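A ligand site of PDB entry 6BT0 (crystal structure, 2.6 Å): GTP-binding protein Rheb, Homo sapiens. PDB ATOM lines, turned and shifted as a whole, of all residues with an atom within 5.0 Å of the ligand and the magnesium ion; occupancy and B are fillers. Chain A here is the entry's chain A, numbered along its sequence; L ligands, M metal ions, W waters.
N of Lys 20 is in hydrogen-bond range of O2 of the ligand (3.2 Å). The side-chain amino group (NZ) of Lys 20 lies within salt-bridge range of an oxygen (O2) of the ligand, at 2.7 Å. The side-chain hydroxyl (OG) of Ser 22 is in hydrogen-bond range of an oxygen (O6) of the ligand (2.5 Å). The backbone NH (N) of Ala 151 lies within hydrogen-bond range of an oxygen (O11) of the ligand. N of Ser 21 lies within hydrogen-bond range of O6 of the ligand (3.2 Å). A nitrogen (N2) of the ligand sits at hydrogen-bond distance from the side-chain amide nitrogen of Asn 120, 3.4 Å away. The backbone NH (N) of Ser 17 is in hydrogen-bond range of an oxygen (O3) of the ligand, at 3.2 Å. The backbone NH (N) of Gly 19 is in hydrogen-bond range of an oxygen (O4) of the ligand (3.0 Å). An oxygen (O10) of the ligand sits at hydrogen-bond distance from the backbone carbonyl oxygen (O) of Asp 34 (3.1 Å). N3 of the ligand sits at hydrogen-bond distance from OD1 of Asp 123 (2.7 Å). O6 of the ligand is in hydrogen-bond range of N of Ser 22 (2.6 Å). NZ of Lys 121 lies close to O8 of the ligand (3.5 Å).
The side-chain amide nitrogen (ND2) of Asn 120 lies within hydrogen-bond range of the backbone carbonyl oxygen (O) of Val 18 (2.7 Å). The side-chain hydroxyl (OG) of Ser 150 lies within hydrogen-bond range of the side-chain carboxylate (OD1) of Asp 123, at 3.1 Å. O of Ser 17 sits at hydrogen-bond distance from NZ of Lys 121. The backbone carbonyl oxygen (O) of Ser 149 is in hydrogen-bond range of the backbone NH (N) of Lys 121, at 3.2 Å. N of Ser 150 sits at hydrogen-bond distance from OD1 of Asn 120 (3.5 Å). OD1 of Asp 61 lies within hydrogen-bond range of N of Ser 21 (3.2 Å). The side-chain amide oxygen (OD1) of Asn 120 is in hydrogen-bond range of the side-chain hydroxyl (OG) of Ser 149, at 2.6 Å. N of Lys 152 lies close to OG of Ser 150, 3.2 Å away.
Residues that only touch the ligand: Val 18, Phe 32, Val 33, Tyr 36, Leu 124 and Ser 150. Hydrophobic or aromatic side chains that line the ligand: Phe 32, Leu 124 and Ala 151. Of the 27 residues printed, 16 come within 4 Å of the ligand.
Merely in contact with the magnesium ion: Asp 61. Two residues have an atom within 4 Å of the magnesium ion: Ser 21 and Asp 61.
The magnesium ion is bound by an oxygen (O1) of the ligand, water W3, water W1, water W4, the side-chain hydroxyl of Ser 21 and water W2. The magnesium ion has six donor atoms within binding distance.
Water W4 bridges an oxygen (O5) of the ligand and the backbone carbonyl oxygen (O) of Tyr 36. Water W3 lies within hydrogen-bond range of the side-chain carboxylate (OD1) of Asp 61 (2.5 Å) and the backbone carbonyl oxygen (O) of Thr 62 (3.0 Å). Water W1 bridges O3 of the ligand (2.8 Å) and O of Ala 63 (2.8 Å).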
ATOM      1  N   ARG A  16      16.775  -7.784  17.938  1.00  0.00           N
ATOM      2  CA  ARG A  16      17.353  -9.059  17.542  1.00  0.00           C
ATOM      3  C   ARG A  16      16.329 -10.046  18.041  1.00  0.00           C
ATOM      4  O   ARG A  16      16.063 -10.076  19.238  1.00  0.00           O
ATOM      5  CB  ARG A  16      18.708  -9.365  18.247  1.00  0.00           C
ATOM      6  CG  ARG A  16      19.964  -8.541  17.896  1.00  0.00           C
ATOM      7  CD  ARG A  16      21.303  -9.312  18.035  1.00  0.00           C
ATOM      8  NE  ARG A  16      21.908  -9.383  19.378  1.00  0.00           N
ATOM      9  CZ  ARG A  16      21.576 -10.229  20.363  1.00  0.00           C
ATOM     10  NH1 ARG A  16      20.578 -11.120  20.238  1.00  0.00           N
ATOM     11  NH2 ARG A  16      22.253 -10.200  21.514  1.00  0.00           N
ATOM     12  N   SER A  17      15.745 -10.800  17.132  1.00  0.00           N
ATOM     13  CA  SER A  17      14.761 -11.835  17.460  1.00  0.00           C
ATOM     14  C   SER A  17      13.429 -11.315  18.075  1.00  0.00           C
ATOM     15  O   SER A  17      12.726 -12.060  18.722  1.00  0.00           O
ATOM     16  CB  SER A  17      15.398 -12.903  18.361  1.00  0.00           C
ATOM     17  OG  SER A  17      16.750 -13.175  17.973  1.00  0.00           O
ATOM     18  N   VAL A  18      13.089 -10.053  17.831  1.00  0.00           N
ATOM     19  CA  VAL A  18      11.777  -9.501  18.193  1.00  0.00           C
ATOM     20  C   VAL A  18      10.728  -9.687  17.104  1.00  0.00           C
ATOM     21  O   VAL A  18       9.563  -9.281  17.271  1.00  0.00           O
ATOM     22  CB  VAL A  18      11.821  -7.983  18.475  1.00  0.00           C
ATOM     23  CG1 VAL A  18      12.847  -7.681  19.557  1.00  0.00           C
ATOM     24  CG2 VAL A  18      12.059  -7.174  17.193  1.00  0.00           C
ATOM     25  N   GLY A  19      11.114 -10.252  15.981  1.00  0.00           N
ATOM     26  CA  GLY A  19      10.129 -10.626  14.978  1.00  0.00           C
ATOM     27  C   GLY A  19      10.002  -9.722  13.783  1.00  0.00           C
ATOM     28  O   GLY A  19       9.018  -9.796  13.102  1.00  0.00           O
ATOM     29  N   LYS A  20      11.006  -8.916  13.485  1.00  0.00           N
ATOM     30  CA  LYS A  20      10.946  -8.007  12.355  1.00  0.00           C
ATOM     31  C   LYS A  20      10.621  -8.757  11.053  1.00  0.00           C
ATOM     32  O   LYS A  20       9.666  -8.423  10.330  1.00  0.00           O
ATOM     33  CB  LYS A  20      12.275  -7.298  12.210  1.00  0.00           C
ATOM     34  CG  LYS A  20      12.683  -6.485  13.426  1.00  0.00           C
ATOM     35  CD  LYS A  20      13.958  -5.663  13.243  1.00  0.00           C
ATOM     36  CE  LYS A  20      15.162  -6.482  12.819  1.00  0.00           C
ATOM     37  NZ  LYS A  20      15.601  -7.409  13.875  1.00  0.00           N
ATOM     38  N   SER A  21      11.398  -9.788  10.781  1.00  0.00           N
ATOM     39  CA  SER A  21      11.253 -10.595   9.585  1.00  0.00           C
ATOM     40  C   SER A  21       9.923 -11.319   9.611  1.00  0.00           C
ATOM     41  O   SER A  21       9.142 -11.220   8.650  1.00  0.00           O
ATOM     42  CB  SER A  21      12.382 -11.615   9.479  1.00  0.00           C
ATOM     43  OG  SER A  21      13.672 -11.001   9.467  1.00  0.00           O
ATOM     44  N   SER A  22       9.629 -11.992  10.722  1.00  0.00           N
ATOM     45  CA  SER A  22       8.430 -12.812  10.789  1.00  0.00           C
ATOM     46  C   SER A  22       7.154 -12.009  10.558  1.00  0.00           C
ATOM     47  O   SER A  22       6.245 -12.447   9.817  1.00  0.00           O
ATOM     48  CB  SER A  22       8.415 -13.571  12.115  1.00  0.00           C
ATOM     49  OG  SER A  22       9.684 -14.180  12.336  1.00  0.00           O
ATOM     50  N   LEU A  23       7.115 -10.818  11.177  1.00  0.00           N
ATOM     51  CA  LEU A  23       6.007  -9.835  11.048  1.00  0.00           C
ATOM     52  C   LEU A  23       5.860  -9.314   9.593  1.00  0.00           C
ATOM     53  O   LEU A  23       4.774  -9.283   9.047  1.00  0.00           O
ATOM     54  CB  LEU A  23       6.275  -8.644  11.959  1.00  0.00           C
ATOM     55  CG  LEU A  23       5.194  -7.929  12.759  1.00  0.00           C
ATOM     56  CD1 LEU A  23       5.465  -6.415  12.775  1.00  0.00           C
ATOM     57  CD2 LEU A  23       3.801  -8.223  12.251  1.00  0.00           C
ATOM     58  N   PHE A  32       3.302 -17.177   8.519  1.00  0.00           N
ATOM     59  CA  PHE A  32       4.268 -17.185   9.621  1.00  0.00           C
ATOM     60  C   PHE A  32       5.378 -18.211   9.358  1.00  0.00           C
ATOM     61  O   PHE A  32       5.099 -19.390   9.181  1.00  0.00           O
ATOM     62  CB  PHE A  32       3.560 -17.558  10.923  1.00  0.00           C
ATOM     63  CG  PHE A  32       4.470 -17.608  12.135  1.00  0.00           C
ATOM     64  CD1 PHE A  32       5.123 -16.457  12.573  1.00  0.00           C
ATOM     65  CD2 PHE A  32       4.651 -18.797  12.831  1.00  0.00           C
ATOM     66  CE1 PHE A  32       5.949 -16.482  13.689  1.00  0.00           C
ATOM     67  CE2 PHE A  32       5.484 -18.837  13.936  1.00  0.00           C
ATOM     68  CZ  PHE A  32       6.130 -17.683  14.366  1.00  0.00           C
ATOM     69  N   VAL A  33       6.635 -17.771   9.345  1.00  0.00           N
ATOM     70  CA  VAL A  33       7.793 -18.663   9.213  1.00  0.00           C
ATOM     71  C   VAL A  33       8.339 -19.117  10.564  1.00  0.00           C
ATOM     72  O   VAL A  33       8.251 -18.393  11.582  1.00  0.00           O
ATOM     73  CB  VAL A  33       8.961 -18.005   8.457  1.00  0.00           C
ATOM     74  CG1 VAL A  33       8.562 -17.633   7.050  1.00  0.00           C
ATOM     75  CG2 VAL A  33       9.531 -16.807   9.236  1.00  0.00           C
ATOM     76  N   ASP A  34       8.978 -20.298  10.545  1.00  0.00           N
ATOM     77  CA  ASP A  34       9.579 -20.923  11.753  1.00  0.00           C
ATOM     78  C   ASP A  34      10.910 -20.304  12.119  1.00  0.00           C
ATOM     79  O   ASP A  34      11.103 -19.915  13.278  1.00  0.00           O
ATOM     80  CB  ASP A  34       9.747 -22.443  11.611  1.00  0.00           C
ATOM     81  CG  ASP A  34       9.796 -22.923  10.156  1.00  0.00           C
ATOM     82  OD1 ASP A  34       9.649 -22.090   9.229  1.00  0.00           O
ATOM     83  OD2 ASP A  34       9.950 -24.132   9.951  1.00  0.00           O
ATOM     84  N   TYR A  36      13.917 -17.532  10.100  1.00  0.00           N
ATOM     85  CA  TYR A  36      14.415 -16.777   8.980  1.00  0.00           C
ATOM     86  C   TYR A  36      15.786 -16.202   9.392  1.00  0.00           C
ATOM     87  O   TYR A  36      15.987 -15.777  10.542  1.00  0.00           O
ATOM     88  CB  TYR A  36      13.387 -15.710   8.602  1.00  0.00           C
ATOM     89  CG  TYR A  36      13.754 -14.829   7.438  1.00  0.00           C
ATOM     90  CD1 TYR A  36      13.519 -15.218   6.119  1.00  0.00           C
ATOM     91  CD2 TYR A  36      14.330 -13.597   7.661  1.00  0.00           C
ATOM     92  CE1 TYR A  36      13.880 -14.392   5.055  1.00  0.00           C
ATOM     93  CE2 TYR A  36      14.682 -12.757   6.627  1.00  0.00           C
ATOM     94  CZ  TYR A  36      14.467 -13.145   5.317  1.00  0.00           C
ATOM     95  OH  TYR A  36      14.852 -12.266   4.321  1.00  0.00           O
ATOM     96  N   ASP A  37      16.752 -16.251   8.467  1.00  0.00           N
ATOM     97  CA  ASP A  37      18.126 -15.928   8.773  1.00  0.00           C
ATOM     98  C   ASP A  37      18.232 -14.486   9.254  1.00  0.00           C
ATOM     99  O   ASP A  37      17.837 -13.566   8.540  1.00  0.00           O
ATOM    100  CB  ASP A  37      19.005 -16.132   7.531  1.00  0.00           C
ATOM    101  CG  ASP A  37      20.492 -15.959   7.818  1.00  0.00           C
ATOM    102  OD1 ASP A  37      20.887 -14.970   8.491  1.00  0.00           O
ATOM    103  OD2 ASP A  37      21.273 -16.816   7.360  1.00  0.00           O
ATOM    104  N   PRO A  38      18.766 -14.282  10.462  1.00  0.00           N
ATOM    105  CA  PRO A  38      18.880 -12.959  11.066  1.00  0.00           C
ATOM    106  C   PRO A  38      20.089 -12.147  10.599  1.00  0.00           C
ATOM    107  O   PRO A  38      20.362 -11.079  11.173  1.00  0.00           O
ATOM    108  CB  PRO A  38      19.044 -13.280  12.533  1.00  0.00           C
ATOM    109  CG  PRO A  38      19.870 -14.527  12.496  1.00  0.00           C
ATOM    110  CD  PRO A  38      19.330 -15.315  11.346  1.00  0.00           C
ATOM    111  N   ILE A  40      20.093 -11.458   7.259  1.00  0.00           N
ATOM    112  CA  ILE A  40      19.612 -10.941   5.983  1.00  0.00           C
ATOM    113  C   ILE A  40      18.868  -9.618   6.140  1.00  0.00           C
ATOM    114  O   ILE A  40      17.812  -9.560   6.797  1.00  0.00           O
ATOM    115  CB  ILE A  40      18.677 -11.943   5.298  1.00  0.00           C
ATOM    116  CG1 ILE A  40      19.433 -13.251   4.991  1.00  0.00           C
ATOM    117  CG2 ILE A  40      18.059 -11.321   4.033  1.00  0.00           C
ATOM    118  CD1 ILE A  40      18.558 -14.406   4.553  1.00  0.00           C
ATOM    119  N   ASP A  61      13.577  -5.046   5.736  1.00  0.00           N
ATOM    120  CA  ASP A  61      13.701  -5.903   6.922  1.00  0.00           C
ATOM    121  C   ASP A  61      15.144  -5.930   7.440  1.00  0.00           C
ATOM    122  O   ASP A  61      15.890  -6.872   7.157  1.00  0.00           O
ATOM    123  CB  ASP A  61      13.230  -7.333   6.598  1.00  0.00           C
ATOM    124  CG  ASP A  61      13.310  -8.271   7.811  1.00  0.00           C
ATOM    125  OD1 ASP A  61      13.181  -7.825   8.973  1.00  0.00           O
ATOM    126  OD2 ASP A  61      13.504  -9.484   7.566  1.00  0.00           O
ATOM    127  N   THR A  62      15.536  -4.913   8.197  1.00  0.00           N
ATOM    128  CA  THR A  62      16.937  -4.754   8.591  1.00  0.00           C
ATOM    129  C   THR A  62      17.462  -5.931   9.345  1.00  0.00           C
ATOM    130  O   THR A  62      16.703  -6.633   9.991  1.00  0.00           O
ATOM    131  CB  THR A  62      17.171  -3.530   9.474  1.00  0.00           C
ATOM    132  OG1 THR A  62      16.422  -3.629  10.712  1.00  0.00           O
ATOM    133  CG2 THR A  62      16.786  -2.283   8.709  1.00  0.00           C
ATOM    134  N   ALA A  63      18.762  -6.140   9.276  1.00  0.00           N
ATOM    135  CA  ALA A  63      19.403  -7.279   9.960  1.00  0.00           C
ATOM    136  C   ALA A  63      19.140  -7.250  11.462  1.00  0.00           C
ATOM    137  O   ALA A  63      18.860  -8.283  12.043  1.00  0.00           O
ATOM    138  CB  ALA A  63      20.910  -7.302   9.684  1.00  0.00           C
ATOM    139  N   ASN A 120       5.575  -6.406  19.688  1.00  0.00           N
ATOM    140  CA  ASN A 120       5.340  -7.668  19.007  1.00  0.00           C
ATOM    141  C   ASN A 120       5.431  -8.845  19.982  1.00  0.00           C
ATOM    142  O   ASN A 120       5.904  -8.703  21.098  1.00  0.00           O
ATOM    143  CB  ASN A 120       6.367  -7.828  17.897  1.00  0.00           C
ATOM    144  CG  ASN A 120       6.002  -8.887  16.883  1.00  0.00           C
ATOM    145  OD1 ASN A 120       4.869  -8.956  16.404  1.00  0.00           O
ATOM    146  ND2 ASN A 120       6.964  -9.747  16.564  1.00  0.00           N
ATOM    147  N   LYS A 121       4.958 -10.000  19.512  1.00  0.00           N
ATOM    148  CA  LYS A 121       4.873 -11.260  20.254  1.00  0.00           C
ATOM    149  C   LYS A 121       3.755 -11.214  21.269  1.00  0.00           C
ATOM    150  O   LYS A 121       3.827 -11.892  22.282  1.00  0.00           O
ATOM    151  CB  LYS A 121       6.204 -11.657  20.907  1.00  0.00           C
ATOM    152  CG  LYS A 121       7.397 -11.671  19.961  1.00  0.00           C
ATOM    153  CD  LYS A 121       8.492 -12.639  20.424  1.00  0.00           C
ATOM    154  CE  LYS A 121       9.586 -12.794  19.379  1.00  0.00           C
ATOM    155  NZ  LYS A 121      10.867 -13.162  20.019  1.00  0.00           N
ATOM    156  N   LYS A 122       2.698 -10.450  20.970  1.00  0.00           N
ATOM    157  CA  LYS A 122       1.576 -10.305  21.909  1.00  0.00           C
ATOM    158  C   LYS A 122       0.842 -11.629  22.179  1.00  0.00           C
ATOM    159  O   LYS A 122       0.197 -11.780  23.197  1.00  0.00           O
ATOM    160  CB  LYS A 122       0.601  -9.202  21.478  1.00  0.00           C
ATOM    161  CG  LYS A 122      -0.425  -9.582  20.426  1.00  0.00           C
ATOM    162  CD  LYS A 122      -1.203  -8.354  19.963  1.00  0.00           C
ATOM    163  CE  LYS A 122      -2.396  -8.739  19.115  1.00  0.00           C
ATOM    164  NZ  LYS A 122      -3.631  -9.089  19.887  1.00  0.00           N
ATOM    165  N   ASP A 123       0.985 -12.595  21.295  1.00  0.00           N
ATOM    166  CA  ASP A 123       0.376 -13.903  21.478  1.00  0.00           C
ATOM    167  C   ASP A 123       0.916 -14.736  22.642  1.00  0.00           C
ATOM    168  O   ASP A 123       0.336 -15.779  22.949  1.00  0.00           O
ATOM    169  CB  ASP A 123       0.485 -14.717  20.192  1.00  0.00           C
ATOM    170  CG  ASP A 123       1.904 -14.980  19.829  1.00  0.00           C
ATOM    171  OD1 ASP A 123       2.587 -13.966  19.498  1.00  0.00           O
ATOM    172  OD2 ASP A 123       2.347 -16.167  19.897  1.00  0.00           O
ATOM    173  N   LEU A 124       2.001 -14.323  23.290  1.00  0.00           N
ATOM    174  CA  LEU A 124       2.590 -15.103  24.397  1.00  0.00           C
ATOM    175  C   LEU A 124       2.163 -14.597  25.796  1.00  0.00           C
ATOM    176  O   LEU A 124       2.969 -14.058  26.572  1.00  0.00           O
ATOM    177  CB  LEU A 124       4.108 -15.163  24.225  1.00  0.00           C
ATOM    178  CG  LEU A 124       4.586 -15.848  22.929  1.00  0.00           C
ATOM    179  CD1 LEU A 124       6.059 -15.561  22.580  1.00  0.00           C
ATOM    180  CD2 LEU A 124       4.323 -17.357  22.979  1.00  0.00           C
ATOM    181  N   SER A 149       1.424  -6.212  18.176  1.00  0.00           N
ATOM    182  CA  SER A 149       1.344  -7.147  17.059  1.00  0.00           C
ATOM    183  C   SER A 149       1.678  -8.588  17.459  1.00  0.00           C
ATOM    184  O   SER A 149       2.125  -8.882  18.604  1.00  0.00           O
ATOM    185  CB  SER A 149       2.305  -6.727  15.960  1.00  0.00           C
ATOM    186  OG  SER A 149       3.627  -6.639  16.434  1.00  0.00           O
ATOM    187  N   SER A 150       1.417  -9.475  16.506  1.00  0.00           N
ATOM    188  CA  SER A 150       1.830 -10.856  16.549  1.00  0.00           C
ATOM    189  C   SER A 150       2.060 -11.261  15.132  1.00  0.00           C
ATOM    190  O   SER A 150       1.184 -11.063  14.284  1.00  0.00           O
ATOM    191  CB  SER A 150       0.727 -11.731  17.136  1.00  0.00           C
ATOM    192  OG  SER A 150       1.038 -13.125  17.000  1.00  0.00           O
ATOM    193  N   ALA A 151       3.220 -11.836  14.852  1.00  0.00           N
ATOM    194  CA  ALA A 151       3.485 -12.376  13.527  1.00  0.00           C
ATOM    195  C   ALA A 151       2.654 -13.636  13.195  1.00  0.00           C
ATOM    196  O   ALA A 151       2.454 -13.950  12.041  1.00  0.00           O
ATOM    197  CB  ALA A 151       4.983 -12.638  13.361  1.00  0.00           C
ATOM    198  N   LYS A 152       2.189 -14.359  14.223  1.00  0.00           N
ATOM    199  CA  LYS A 152       1.233 -15.449  14.016  1.00  0.00           C
ATOM    200  C   LYS A 152      -0.065 -14.925  13.390  1.00  0.00           C
ATOM    201  O   LYS A 152      -0.576 -15.518  12.453  1.00  0.00           O
ATOM    202  CB  LYS A 152       0.918 -16.190  15.323  1.00  0.00           C
ATOM    203  CG  LYS A 152       2.125 -16.888  15.932  1.00  0.00           C
ATOM    204  CD  LYS A 152       1.741 -18.095  16.782  1.00  0.00           C
ATOM    205  CE  LYS A 152       2.906 -19.085  16.967  1.00  0.00           C
ATOM    206  NZ  LYS A 152       2.563 -20.234  17.870  1.00  0.00           N
HETATM  207  P1  LIG L   1      14.215 -10.789  13.732  1.00  0.00           P
HETATM  208  O1  LIG L   1      13.908 -10.775  12.252  1.00  0.00           O
HETATM  209  O2  LIG L   1      13.997  -9.464  14.457  1.00  0.00           O
HETATM  210  O3  LIG L   1      15.538 -11.405  14.026  1.00  0.00           O
HETATM  211  O4  LIG L   1      13.079 -11.771  14.370  1.00  0.00           O
HETATM  212  P2  LIG L   1      12.388 -12.951  13.499  1.00  0.00           P
HETATM  213  O5  LIG L   1      13.554 -13.662  12.863  1.00  0.00           O
HETATM  214  O6  LIG L   1      11.312 -12.360  12.654  1.00  0.00           O
HETATM  215  O7  LIG L   1      11.683 -13.934  14.553  1.00  0.00           O
HETATM  216  C1  LIG L   1      12.440 -14.192  15.739  1.00  0.00           C
HETATM  217  C2  LIG L   1      12.002 -15.459  16.462  1.00  0.00           C
HETATM  218  O8  LIG L   1      10.820 -15.225  17.203  1.00  0.00           O
HETATM  219  C3  LIG L   1      11.657 -16.599  15.529  1.00  0.00           C
HETATM  220  O9  LIG L   1      11.978 -17.828  16.219  1.00  0.00           O
HETATM  221  C4  LIG L   1      10.181 -16.442  15.291  1.00  0.00           C
HETATM  222  O10 LIG L   1       9.654 -17.727  14.973  1.00  0.00           O
HETATM  223  C5  LIG L   1       9.707 -15.881  16.627  1.00  0.00           C
HETATM  224  N1  LIG L   1       8.586 -14.889  16.585  1.00  0.00           N
HETATM  225  C6  LIG L   1       8.556 -13.715  15.939  1.00  0.00           C
HETATM  226  N2  LIG L   1       7.378 -13.058  16.121  1.00  0.00           N
HETATM  227  C7  LIG L   1       6.641 -13.812  16.914  1.00  0.00           C
HETATM  228  C8  LIG L   1       5.321 -13.712  17.525  1.00  0.00           C
HETATM  229  O11 LIG L   1       4.592 -12.718  17.320  1.00  0.00           O
HETATM  230  N3  LIG L   1       4.910 -14.713  18.302  1.00  0.00           N
HETATM  231  C9  LIG L   1       5.652 -15.798  18.562  1.00  0.00           C
HETATM  232  N4  LIG L   1       5.148 -16.779  19.364  1.00  0.00           N
HETATM  233  N5  LIG L   1       6.906 -15.943  18.042  1.00  0.00           N
HETATM  234  C10 LIG L   1       7.431 -15.003  17.234  1.00  0.00           C
HETATM  235 MG    MG M   1      15.265 -10.908  10.845  1.00  0.00          MG
HETATM  236  O   HOH W   1      16.860 -10.248  11.875  1.00  0.00           O
HETATM  237  O   HOH W   2      16.622 -11.137   9.131  1.00  0.00           O
HETATM  238  O   HOH W   3      14.982  -9.042  10.272  1.00  0.00           O
HETATM  239  O   HOH W   4      15.234 -12.972  11.133  1.00  0.00           O
